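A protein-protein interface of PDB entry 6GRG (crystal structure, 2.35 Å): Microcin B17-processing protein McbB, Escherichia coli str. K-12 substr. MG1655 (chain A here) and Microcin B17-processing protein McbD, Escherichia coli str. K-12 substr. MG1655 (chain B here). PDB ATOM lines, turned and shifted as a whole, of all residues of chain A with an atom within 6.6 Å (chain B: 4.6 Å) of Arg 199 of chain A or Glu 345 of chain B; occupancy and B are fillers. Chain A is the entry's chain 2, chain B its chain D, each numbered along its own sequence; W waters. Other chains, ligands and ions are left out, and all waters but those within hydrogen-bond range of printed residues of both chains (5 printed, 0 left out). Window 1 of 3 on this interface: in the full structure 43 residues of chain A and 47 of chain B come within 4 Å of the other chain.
The backbone carbonyl oxygen (O) of Glu 345 of chain B lies within hydrogen-bond range of the backbone NH (N) of Val 352 of chain B (2.9 Å).
The side-chain sulfur (SG) of Cys 195 of chain A sits close to the backbone NH (N) of Trp 287 of chain A, at 3.6 Å.
NH1 of Arg 199 of chain A sits at hydrogen-bond distance from O of His 286 of chain A.
ND1 of His 286 of chain A lies close to SG of Cys 195 of chain A (3.7 Å).
The side-chain carboxylate (OE2) of Glu 67 of chain B is in salt-bridge range of the guanidinium group (NE) of Arg 62 of chain B, at 3.0 Å.
Among the printed residues, merely in contact across the chains: His 286 of chain A with Glu 345 of chain B, Ile 285 of chain A with Arg 346 of chain B, Trp 287 of chain A with Glu 67 of chain B, Trp 287 of chain A with Glu 345 of chain B, Arg 203 of chain A with Arg 62 of chain B, Ile 285 of chain A with Val 347 of chain B, Tyr 32 of chain A with Arg 344 of chain B, Tyr 32 of chain A with Leu 351 of chain B and Ser 202 of chain A with Glu 67 of chain B.
Water W1 lies within hydrogen-bond range of OE2 of Glu 345 of chain B (2.5 Å), OE1 of Glu 67 of chain B (2.6 Å) and NH2 of Arg 199 of chain A (3.3 Å).
Water W4 bridges O of Arg 344 of chain B and O of Tyr 32 of chain A.
Water W2 bridges OE2 of Glu 67 of chain B (2.8 Å) and O of Arg 199 of chain A (3.4 Å).
Water W3 lies within hydrogen-bond range of the backbone carbonyl oxygen of Glu 67 of chain B and the indole nitrogen of Trp 287 of chain A.
Water W5 lies within hydrogen-bond range of the side-chain carboxylate (OE1) of Glu 67 of chain B (3.1 Å), the guanidinium group (NE) of Arg 62 of chain B (3.1 Å), the side-chain hydroxyl (OH) of Tyr 354 of chain B (3.3 Å) and the guanidinium group (NH2) of Arg 199 of chain A (3.5 Å).
Printed residues of chain B that touch a printed residue of chain A: Arg 62, Glu 67, Arg 344, Glu 345, Arg 346, Val 347, Leu 351 and Tyr 354.
Hydrophobic or aromatic side chains of chain B that line the printed part of chain A: Val 347, Leu 351 and Tyr 354.
Along chain B the printed residues that touch a printed residue of chain A span positions 62 to 354.
Hydrophobic or aromatic side chains of chain A that line the printed part of chain B: Tyr 32, Ile 285, His 286 and Trp 287.
Among the printed residues, 16 pairs touch across the chains.
Among the printed residues, Asp or Glu carboxylates within 4 Å of a Lys or Arg side-chain nitrogen of the other chain: Arg 199 of chain A with Glu 67 of chain B (2.7 Å) and Arg 199 of chain A with Glu 345 of chain B (2.8 Å).
NH2 of Arg 199 of chain A sits at hydrogen-bond distance from OH of Tyr 354 of chain B (3.3 Å).
The guanidinium group of Arg 62 of chain B lies close to the guanidinium group of Arg 199 of chain A.
The guanidinium group of Arg 199 of chain A lies within salt-bridge range of the side-chain carboxylate of Glu 345 of chain B, 2.8 Å away.
OE2 of Glu 345 of chain B sits at hydrogen-bond distance from N of Gln 288 of chain A (3.1 Å).
The side-chain amide oxygen (OE1) of Gln 288 of chain A sits at hydrogen-bond distance from the guanidinium group (NH1) of Arg 344 of chain B, at 2.8 Å.
The guanidinium group (NE) of Arg 199 of chain A is in salt-bridge range of the side-chain carboxylate (OE2) of Glu 67 of chain B, at 2.7 Å.
N of His 286 of chain A is in hydrogen-bond range of O of Arg 346 of chain B (3.1 Å).
Of chain A, only Arg 199 (2.8 Å), His 286 (3.3 Å), Trp 287 (3.6 Å) and Gln 288 (3.1 Å) come within 4 Å of Glu 345 of chain B.
Printed residues of chain A within 4 Å of Arg 346 of chain B: Ile 285 (3.4 Å) and His 286 (3.1 Å).
Of the printed residues of chain B, His 286 of chain A touches Glu 345 (3.3 Å) and Arg 346 (3.1 Å).
Printed residues of chain B within 4 Å of Ile 285 of chain A: Arg 346 (3.4 Å) and Val 347 (3.6 Å).
The nearest residue of chain A that does not touch Glu 345 of chain B is Ile 285 of chain A (4.1 Å).
The nearest printed residue of chain A that does not touch Leu 351 of chain B is His 286 of chain A (6.7 Å).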
ATOM      1  N   TYR A  32      -4.052  19.653   6.491  1.00  0.00           N
ATOM      2  CA  TYR A  32      -3.069  20.057   5.535  1.00  0.00           C
ATOM      3  C   TYR A  32      -1.691  19.461   5.874  1.00  0.00           C
ATOM      4  O   TYR A  32      -0.891  19.331   4.964  1.00  0.00           O
ATOM      5  CB  TYR A  32      -3.098  21.576   5.370  1.00  0.00           C
ATOM      6  CG  TYR A  32      -2.308  22.390   6.365  1.00  0.00           C
ATOM      7  CD1 TYR A  32      -2.609  22.409   7.718  1.00  0.00           C
ATOM      8  CD2 TYR A  32      -1.277  23.202   5.921  1.00  0.00           C
ATOM      9  CE1 TYR A  32      -1.891  23.199   8.600  1.00  0.00           C
ATOM     10  CE2 TYR A  32      -0.552  23.994   6.791  1.00  0.00           C
ATOM     11  CZ  TYR A  32      -0.860  23.991   8.128  1.00  0.00           C
ATOM     12  OH  TYR A  32      -0.114  24.793   8.939  1.00  0.00           O
ATOM     13  N   PHE A 194       9.443  28.588  -1.652  1.00  0.00           N
ATOM     14  CA  PHE A 194       9.846  27.349  -2.324  1.00  0.00           C
ATOM     15  C   PHE A 194       8.636  26.605  -2.878  1.00  0.00           C
ATOM     16  O   PHE A 194       8.765  25.901  -3.840  1.00  0.00           O
ATOM     17  CB  PHE A 194      10.657  26.458  -1.380  1.00  0.00           C
ATOM     18  CG  PHE A 194      11.949  27.112  -0.985  1.00  0.00           C
ATOM     19  CD1 PHE A 194      13.023  27.113  -1.858  1.00  0.00           C
ATOM     20  CD2 PHE A 194      12.034  27.849   0.187  1.00  0.00           C
ATOM     21  CE1 PHE A 194      14.188  27.784  -1.529  1.00  0.00           C
ATOM     22  CE2 PHE A 194      13.195  28.530   0.510  1.00  0.00           C
ATOM     23  CZ  PHE A 194      14.277  28.483  -0.343  1.00  0.00           C
ATOM     24  N   CYS A 195       7.495  26.710  -2.205  1.00  0.00           N
ATOM     25  CA  CYS A 195       6.230  26.227  -2.718  1.00  0.00           C
ATOM     26  C   CYS A 195       5.982  26.738  -4.146  1.00  0.00           C
ATOM     27  O   CYS A 195       5.177  26.139  -4.847  1.00  0.00           O
ATOM     28  CB  CYS A 195       5.054  26.738  -1.893  1.00  0.00           C
ATOM     29  SG  CYS A 195       4.709  25.775  -0.408  1.00  0.00           S
ATOM     30  N   HIS A 196       6.558  27.891  -4.528  1.00  0.00           N
ATOM     31  CA  HIS A 196       6.429  28.377  -5.910  1.00  0.00           C
ATOM     32  C   HIS A 196       7.557  27.827  -6.791  1.00  0.00           C
ATOM     33  O   HIS A 196       7.325  27.026  -7.730  1.00  0.00           O
ATOM     34  CB  HIS A 196       6.400  29.912  -5.989  1.00  0.00           C
ATOM     35  CG  HIS A 196       6.555  30.414  -7.390  1.00  0.00           C
ATOM     36  ND1 HIS A 196       5.592  30.198  -8.365  1.00  0.00           N
ATOM     37  CD2 HIS A 196       7.562  31.079  -7.999  1.00  0.00           C
ATOM     38  CE1 HIS A 196       5.999  30.719  -9.510  1.00  0.00           C
ATOM     39  NE2 HIS A 196       7.202  31.273  -9.312  1.00  0.00           N
ATOM     40  N   ILE A 197       8.778  28.281  -6.489  1.00  0.00           N
ATOM     41  CA  ILE A 197       9.926  28.125  -7.397  1.00  0.00           C
ATOM     42  C   ILE A 197      10.418  26.656  -7.481  1.00  0.00           C
ATOM     43  O   ILE A 197      10.689  26.177  -8.586  1.00  0.00           O
ATOM     44  CB  ILE A 197      11.031  29.134  -7.022  1.00  0.00           C
ATOM     45  CG1 ILE A 197      12.165  29.110  -8.048  1.00  0.00           C
ATOM     46  CG2 ILE A 197      11.545  28.936  -5.601  1.00  0.00           C
ATOM     47  CD1 ILE A 197      13.003  30.373  -8.039  1.00  0.00           C
ATOM     48  N   GLU A 198      10.494  25.935  -6.345  1.00  0.00           N
ATOM     49  CA  GLU A 198      10.913  24.524  -6.306  1.00  0.00           C
ATOM     50  C   GLU A 198       9.884  23.683  -7.060  1.00  0.00           C
ATOM     51  O   GLU A 198      10.238  22.736  -7.740  1.00  0.00           O
ATOM     52  CB  GLU A 198      11.043  23.950  -4.889  1.00  0.00           C
ATOM     53  CG  GLU A 198      12.406  24.145  -4.247  1.00  0.00           C
ATOM     54  CD  GLU A 198      13.566  23.868  -5.187  1.00  0.00           C
ATOM     55  OE1 GLU A 198      13.668  22.711  -5.662  1.00  0.00           O
ATOM     56  OE2 GLU A 198      14.339  24.818  -5.490  1.00  0.00           O
ATOM     57  N   ARG A 199       8.604  24.026  -6.909  1.00  0.00           N
ATOM     58  CA  ARG A 199       7.558  23.338  -7.653  1.00  0.00           C
ATOM     59  C   ARG A 199       7.709  23.642  -9.149  1.00  0.00           C
ATOM     60  O   ARG A 199       7.562  22.756  -9.961  1.00  0.00           O
ATOM     61  CB  ARG A 199       6.173  23.738  -7.141  1.00  0.00           C
ATOM     62  CG  ARG A 199       5.020  23.017  -7.825  1.00  0.00           C
ATOM     63  CD  ARG A 199       3.713  23.384  -7.147  1.00  0.00           C
ATOM     64  NE  ARG A 199       2.604  22.572  -7.621  1.00  0.00           N
ATOM     65  CZ  ARG A 199       1.481  22.379  -6.956  1.00  0.00           C
ATOM     66  NH1 ARG A 199       1.302  22.958  -5.776  1.00  0.00           N
ATOM     67  NH2 ARG A 199       0.550  21.608  -7.486  1.00  0.00           N
ATOM     68  N   TRP A 200       8.024  24.900  -9.484  1.00  0.00           N
ATOM     69  CA  TRP A 200       8.238  25.323 -10.869  1.00  0.00           C
ATOM     70  C   TRP A 200       9.389  24.534 -11.502  1.00  0.00           C
ATOM     71  O   TRP A 200       9.288  24.129 -12.668  1.00  0.00           O
ATOM     72  CB  TRP A 200       8.495  26.835 -10.959  1.00  0.00           C
ATOM     73  CG  TRP A 200       8.437  27.339 -12.368  1.00  0.00           C
ATOM     74  CD1 TRP A 200       7.334  27.762 -13.054  1.00  0.00           C
ATOM     75  CD2 TRP A 200       9.537  27.441 -13.286  1.00  0.00           C
ATOM     76  NE1 TRP A 200       7.671  28.122 -14.332  1.00  0.00           N
ATOM     77  CE2 TRP A 200       9.017  27.951 -14.499  1.00  0.00           C
ATOM     78  CE3 TRP A 200      10.909  27.154 -13.199  1.00  0.00           C
ATOM     79  CZ2 TRP A 200       9.823  28.145 -15.619  1.00  0.00           C
ATOM     80  CZ3 TRP A 200      11.704  27.363 -14.302  1.00  0.00           C
ATOM     81  CH2 TRP A 200      11.165  27.847 -15.497  1.00  0.00           C
ATOM     82  N   LEU A 201      10.492  24.378 -10.748  1.00  0.00           N
ATOM     83  CA  LEU A 201      11.692  23.618 -11.194  1.00  0.00           C
ATOM     84  C   LEU A 201      11.358  22.130 -11.313  1.00  0.00           C
ATOM     85  O   LEU A 201      11.728  21.502 -12.304  1.00  0.00           O
ATOM     86  CB  LEU A 201      12.857  23.845 -10.229  1.00  0.00           C
ATOM     87  CG  LEU A 201      13.494  25.233 -10.330  1.00  0.00           C
ATOM     88  CD1 LEU A 201      14.519  25.475  -9.219  1.00  0.00           C
ATOM     89  CD2 LEU A 201      14.104  25.434 -11.711  1.00  0.00           C
ATOM     90  N   SER A 202      10.645  21.580 -10.322  1.00  0.00           N
ATOM     91  CA  SER A 202      10.170  20.205 -10.417  1.00  0.00           C
ATOM     92  C   SER A 202       9.461  20.001 -11.766  1.00  0.00           C
ATOM     93  O   SER A 202       9.751  19.041 -12.496  1.00  0.00           O
ATOM     94  CB  SER A 202       9.287  19.836  -9.248  1.00  0.00           C
ATOM     95  OG  SER A 202       8.709  18.547  -9.432  1.00  0.00           O
ATOM     96  N   ARG A 203       8.569  20.933 -12.128  1.00  0.00           N
ATOM     97  CA  ARG A 203       7.760  20.764 -13.330  1.00  0.00           C
ATOM     98  C   ARG A 203       8.660  20.796 -14.576  1.00  0.00           C
ATOM     99  O   ARG A 203       8.400  20.061 -15.516  1.00  0.00           O
ATOM    100  CB  ARG A 203       6.603  21.770 -13.357  1.00  0.00           C
ATOM    101  CG  ARG A 203       5.518  21.462 -14.388  1.00  0.00           C
ATOM    102  CD  ARG A 203       4.423  22.524 -14.516  1.00  0.00           C
ATOM    103  NE  ARG A 203       4.939  23.886 -14.670  1.00  0.00           N
ATOM    104  CZ  ARG A 203       4.232  25.006 -14.494  1.00  0.00           C
ATOM    105  NH1 ARG A 203       2.915  24.958 -14.388  1.00  0.00           N
ATOM    106  NH2 ARG A 203       4.855  26.171 -14.444  1.00  0.00           N
ATOM    107  N   GLU A 204       9.717  21.626 -14.578  1.00  0.00           N
ATOM    108  CA  GLU A 204      10.664  21.663 -15.711  1.00  0.00           C
ATOM    109  C   GLU A 204      11.462  20.347 -15.745  1.00  0.00           C
ATOM    110  O   GLU A 204      11.567  19.719 -16.780  1.00  0.00           O
ATOM    111  CB  GLU A 204      11.637  22.843 -15.638  1.00  0.00           C
ATOM    112  CG  GLU A 204      11.063  24.205 -15.982  1.00  0.00           C
ATOM    113  CD  GLU A 204      10.124  24.281 -17.175  1.00  0.00           C
ATOM    114  OE1 GLU A 204      10.600  24.364 -18.357  1.00  0.00           O
ATOM    115  OE2 GLU A 204       8.903  24.287 -16.909  1.00  0.00           O
ATOM    116  N   ILE A 285      -0.502  28.717  -4.091  1.00  0.00           N
ATOM    117  CA  ILE A 285      -1.012  27.566  -3.387  1.00  0.00           C
ATOM    118  C   ILE A 285       0.149  26.767  -2.770  1.00  0.00           C
ATOM    119  O   ILE A 285       1.316  26.975  -3.072  1.00  0.00           O
ATOM    120  CB  ILE A 285      -1.884  26.717  -4.320  1.00  0.00           C
ATOM    121  CG1 ILE A 285      -1.046  25.968  -5.351  1.00  0.00           C
ATOM    122  CG2 ILE A 285      -2.954  27.573  -4.978  1.00  0.00           C
ATOM    123  CD1 ILE A 285      -1.863  24.976  -6.143  1.00  0.00           C
ATOM    124  N   HIS A 286      -0.212  25.878  -1.847  1.00  0.00           N
ATOM    125  CA  HIS A 286       0.718  24.995  -1.208  1.00  0.00           C
ATOM    126  C   HIS A 286       1.191  23.966  -2.234  1.00  0.00           C
ATOM    127  O   HIS A 286       0.489  23.679  -3.217  1.00  0.00           O
ATOM    128  CB  HIS A 286       0.064  24.330   0.005  1.00  0.00           C
ATOM    129  CG  HIS A 286       0.438  24.937   1.305  1.00  0.00           C
ATOM    130  ND1 HIS A 286       1.751  25.093   1.676  1.00  0.00           N
ATOM    131  CD2 HIS A 286      -0.309  25.382   2.338  1.00  0.00           C
ATOM    132  CE1 HIS A 286       1.799  25.637   2.871  1.00  0.00           C
ATOM    133  NE2 HIS A 286       0.544  25.815   3.302  1.00  0.00           N
ATOM    134  N   TRP A 287       2.398  23.447  -1.996  1.00  0.00           N
ATOM    135  CA  TRP A 287       2.953  22.301  -2.722  1.00  0.00           C
ATOM    136  C   TRP A 287       3.081  21.152  -1.724  1.00  0.00           C
ATOM    137  O   TRP A 287       3.828  21.290  -0.751  1.00  0.00           O
ATOM    138  CB  TRP A 287       4.302  22.663  -3.379  1.00  0.00           C
ATOM    139  CG  TRP A 287       4.863  21.610  -4.286  1.00  0.00           C
ATOM    140  CD1 TRP A 287       4.172  20.760  -5.097  1.00  0.00           C
ATOM    141  CD2 TRP A 287       6.251  21.282  -4.461  1.00  0.00           C
ATOM    142  NE1 TRP A 287       5.027  19.908  -5.747  1.00  0.00           N
ATOM    143  CE2 TRP A 287       6.312  20.218  -5.396  1.00  0.00           C
ATOM    144  CE3 TRP A 287       7.446  21.765  -3.905  1.00  0.00           C
ATOM    145  CZ2 TRP A 287       7.518  19.655  -5.806  1.00  0.00           C
ATOM    146  CZ3 TRP A 287       8.639  21.204  -4.308  1.00  0.00           C
ATOM    147  CH2 TRP A 287       8.671  20.161  -5.243  1.00  0.00           C
ATOM    148  N   GLN A 288       2.337  20.058  -1.961  1.00  0.00           N
ATOM    149  CA  GLN A 288       2.364  18.862  -1.091  1.00  0.00           C
ATOM    150  C   GLN A 288       3.828  18.497  -0.772  1.00  0.00           C
ATOM    151  O   GLN A 288       4.161  18.221   0.373  1.00  0.00           O
ATOM    152  CB  GLN A 288       1.563  17.722  -1.735  1.00  0.00           C
ATOM    153  CG  GLN A 288       1.603  16.374  -0.988  1.00  0.00           C
ATOM    154  CD  GLN A 288       1.006  16.339   0.409  1.00  0.00           C
ATOM    155  OE1 GLN A 288      -0.041  15.734   0.678  1.00  0.00           O
ATOM    156  NE2 GLN A 288       1.706  16.945   1.345  1.00  0.00           N
ATOM    157  N   ALA A 289       4.726  18.579  -1.764  1.00  0.00           N
ATOM    158  CA  ALA A 289       6.126  18.123  -1.589  1.00  0.00           C
ATOM    159  C   ALA A 289       7.005  19.108  -0.803  1.00  0.00           C
ATOM    160  O   ALA A 289       8.103  18.768  -0.454  1.00  0.00           O
ATOM    161  CB  ALA A 289       6.739  17.854  -2.933  1.00  0.00           C
ATOM    162  N   LEU A 293       5.718  22.303   4.899  1.00  0.00           N
ATOM    163  CA  LEU A 293       4.645  21.482   5.535  1.00  0.00           C
ATOM    164  C   LEU A 293       5.273  20.443   6.475  1.00  0.00           C
ATOM    165  O   LEU A 293       4.681  19.407   6.685  1.00  0.00           O
ATOM    166  CB  LEU A 293       3.798  20.809   4.445  1.00  0.00           C
ATOM    167  CG  LEU A 293       3.070  21.765   3.492  1.00  0.00           C
ATOM    168  CD1 LEU A 293       2.552  21.024   2.280  1.00  0.00           C
ATOM    169  CD2 LEU A 293       1.923  22.479   4.190  1.00  0.00           C
ATOM    170  N   ARG B  62      -0.603  17.035 -13.963  1.00  0.00           N
ATOM    171  CA  ARG B  62       0.603  17.764 -13.543  1.00  0.00           C
ATOM    172  C   ARG B  62       1.157  17.103 -12.262  1.00  0.00           C
ATOM    173  O   ARG B  62       2.376  16.981 -12.060  1.00  0.00           O
ATOM    174  CB  ARG B  62       0.287  19.256 -13.360  1.00  0.00           C
ATOM    175  CG  ARG B  62       1.495  20.125 -13.022  1.00  0.00           C
ATOM    176  CD  ARG B  62       1.247  21.615 -12.759  1.00  0.00           C
ATOM    177  NE  ARG B  62       0.333  21.916 -11.655  1.00  0.00           N
ATOM    178  CZ  ARG B  62       0.161  23.121 -11.086  1.00  0.00           C
ATOM    179  NH1 ARG B  62       0.787  24.197 -11.540  1.00  0.00           N
ATOM    180  NH2 ARG B  62      -0.650  23.246 -10.049  1.00  0.00           N
ATOM    181  N   GLU B  67       4.978  16.354 -10.323  1.00  0.00           N
ATOM    182  CA  GLU B  67       5.139  16.988  -8.975  1.00  0.00           C
ATOM    183  C   GLU B  67       5.302  16.026  -7.772  1.00  0.00           C
ATOM    184  O   GLU B  67       5.435  16.502  -6.625  1.00  0.00           O
ATOM    185  CB  GLU B  67       3.952  17.911  -8.739  1.00  0.00           C
ATOM    186  CG  GLU B  67       4.006  19.199  -9.559  1.00  0.00           C
ATOM    187  CD  GLU B  67       2.743  20.056  -9.466  1.00  0.00           C
ATOM    188  OE1 GLU B  67       1.725  19.568  -8.856  1.00  0.00           O
ATOM    189  OE2 GLU B  67       2.772  21.223  -9.971  1.00  0.00           O
ATOM    190  N   ARG B 344      -2.608  16.298  -0.949  1.00  0.00           N
ATOM    191  CA  ARG B 344      -3.493  17.435  -0.839  1.00  0.00           C
ATOM    192  C   ARG B 344      -2.674  18.715  -0.680  1.00  0.00           C
ATOM    193  O   ARG B 344      -1.536  18.660  -0.205  1.00  0.00           O
ATOM    194  CB  ARG B 344      -4.521  17.213   0.276  1.00  0.00           C
ATOM    195  CG  ARG B 344      -4.003  17.346   1.698  1.00  0.00           C
ATOM    196  CD  ARG B 344      -2.830  16.445   2.023  1.00  0.00           C
ATOM    197  NE  ARG B 344      -2.592  16.321   3.451  1.00  0.00           N
ATOM    198  CZ  ARG B 344      -1.703  15.490   3.973  1.00  0.00           C
ATOM    199  NH1 ARG B 344      -0.859  14.858   3.169  1.00  0.00           N
ATOM    200  NH2 ARG B 344      -1.683  15.266   5.280  1.00  0.00           N
ATOM    201  N   GLU B 345      -3.288  19.834  -1.108  1.00  0.00           N
ATOM    202  CA  GLU B 345      -2.688  21.176  -1.144  1.00  0.00           C
ATOM    203  C   GLU B 345      -3.743  22.213  -0.749  1.00  0.00           C
ATOM    204  O   GLU B 345      -4.866  22.165  -1.255  1.00  0.00           O
ATOM    205  CB  GLU B 345      -2.166  21.485  -2.554  1.00  0.00           C
ATOM    206  CG  GLU B 345      -0.917  20.685  -2.899  1.00  0.00           C
ATOM    207  CD  GLU B 345      -0.435  20.609  -4.342  1.00  0.00           C
ATOM    208  OE1 GLU B 345      -1.140  21.083  -5.263  1.00  0.00           O
ATOM    209  OE2 GLU B 345       0.680  20.079  -4.530  1.00  0.00           O
ATOM    210  N   ARG B 346      -3.357  23.159   0.117  1.00  0.00           N
ATOM    211  CA  ARG B 346      -4.190  24.314   0.427  1.00  0.00           C
ATOM    212  C   ARG B 346      -4.253  25.319  -0.746  1.00  0.00           C
ATOM    213  O   ARG B 346      -3.231  25.713  -1.309  1.00  0.00           O
ATOM    214  CB  ARG B 346      -3.688  25.007   1.691  1.00  0.00           C
ATOM    215  CG  ARG B 346      -4.614  26.108   2.186  1.00  0.00           C
ATOM    216  CD  ARG B 346      -4.162  26.660   3.527  1.00  0.00           C
ATOM    217  NE  ARG B 346      -4.942  27.841   3.865  1.00  0.00           N
ATOM    218  CZ  ARG B 346      -4.968  28.454   5.049  1.00  0.00           C
ATOM    219  NH1 ARG B 346      -4.158  28.110   6.047  1.00  0.00           N
ATOM    220  NH2 ARG B 346      -5.835  29.434   5.207  1.00  0.00           N
ATOM    221  N   VAL B 347      -5.491  25.687  -1.116  1.00  0.00           N
ATOM    222  CA  VAL B 347      -5.857  26.736  -2.083  1.00  0.00           C
ATOM    223  C   VAL B 347      -6.845  27.618  -1.324  1.00  0.00           C
ATOM    224  O   VAL B 347      -7.858  27.136  -0.886  1.00  0.00           O
ATOM    225  CB  VAL B 347      -6.517  26.150  -3.348  1.00  0.00           C
ATOM    226  CG1 VAL B 347      -7.091  27.214  -4.274  1.00  0.00           C
ATOM    227  CG2 VAL B 347      -5.591  25.207  -4.117  1.00  0.00           C
ATOM    228  N   SER B 350      -9.518  26.230   1.370  1.00  0.00           N
ATOM    229  CA  SER B 350      -9.899  24.872   0.977  1.00  0.00           C
ATOM    230  C   SER B 350      -8.646  24.018   0.792  1.00  0.00           C
ATOM    231  O   SER B 350      -7.556  24.532   0.633  1.00  0.00           O
ATOM    232  CB  SER B 350     -10.702  24.879  -0.318  1.00  0.00           C
ATOM    233  OG  SER B 350     -11.707  25.884  -0.276  1.00  0.00           O
ATOM    234  N   LEU B 351      -8.852  22.705   0.770  1.00  0.00           N
ATOM    235  CA  LEU B 351      -7.886  21.759   0.286  1.00  0.00           C
ATOM    236  C   LEU B 351      -8.377  21.236  -1.061  1.00  0.00           C
ATOM    237  O   LEU B 351      -9.569  21.012  -1.217  1.00  0.00           O
ATOM    238  CB  LEU B 351      -7.754  20.615   1.293  1.00  0.00           C
ATOM    239  CG  LEU B 351      -7.150  20.980   2.640  1.00  0.00           C
ATOM    240  CD1 LEU B 351      -7.251  19.810   3.599  1.00  0.00           C
ATOM    241  CD2 LEU B 351      -5.704  21.406   2.483  1.00  0.00           C
ATOM    242  N   VAL B 352      -7.454  21.092  -2.015  1.00  0.00           N
ATOM    243  CA  VAL B 352      -7.671  20.254  -3.192  1.00  0.00           C
ATOM    244  C   VAL B 352      -6.919  18.918  -2.996  1.00  0.00           C
ATOM    245  O   VAL B 352      -5.958  18.823  -2.210  1.00  0.00           O
ATOM    246  CB  VAL B 352      -7.313  20.976  -4.513  1.00  0.00           C
ATOM    247  CG1 VAL B 352      -8.051  22.301  -4.617  1.00  0.00           C
ATOM    248  CG2 VAL B 352      -5.810  21.153  -4.737  1.00  0.00           C
ATOM    249  N   TYR B 354      -5.597  15.029  -4.685  1.00  0.00           N
ATOM    250  CA  TYR B 354      -5.173  14.163  -5.785  1.00  0.00           C
ATOM    251  C   TYR B 354      -5.211  12.728  -5.246  1.00  0.00           C
ATOM    252  O   TYR B 354      -4.579  12.463  -4.222  1.00  0.00           O
ATOM    253  CB  TYR B 354      -3.768  14.535  -6.274  1.00  0.00           C
ATOM    254  CG  TYR B 354      -3.422  16.002  -6.412  1.00  0.00           C
ATOM    255  CD1 TYR B 354      -3.127  16.788  -5.306  1.00  0.00           C
ATOM    256  CD2 TYR B 354      -3.296  16.598  -7.658  1.00  0.00           C
ATOM    257  CE1 TYR B 354      -2.777  18.125  -5.436  1.00  0.00           C
ATOM    258  CE2 TYR B 354      -2.949  17.938  -7.810  1.00  0.00           C
ATOM    259  CZ  TYR B 354      -2.686  18.712  -6.692  1.00  0.00           C
ATOM    260  OH  TYR B 354      -2.333  20.032  -6.836  1.00  0.00           O
HETATM  261  O   HOH W   1       1.445  18.597  -6.447  1.00  0.00           O
HETATM  262  O   HOH W   2       4.406  23.022 -11.319  1.00  0.00           O
HETATM  263  O   HOH W   3       3.357  17.532  -4.897  1.00  0.00           O
HETATM  264  O   HOH W   4      -0.699  19.960   1.988  1.00  0.00           O
HETATM  265  O   HOH W   5      -1.166  19.821  -9.902  1.00  0.00           O
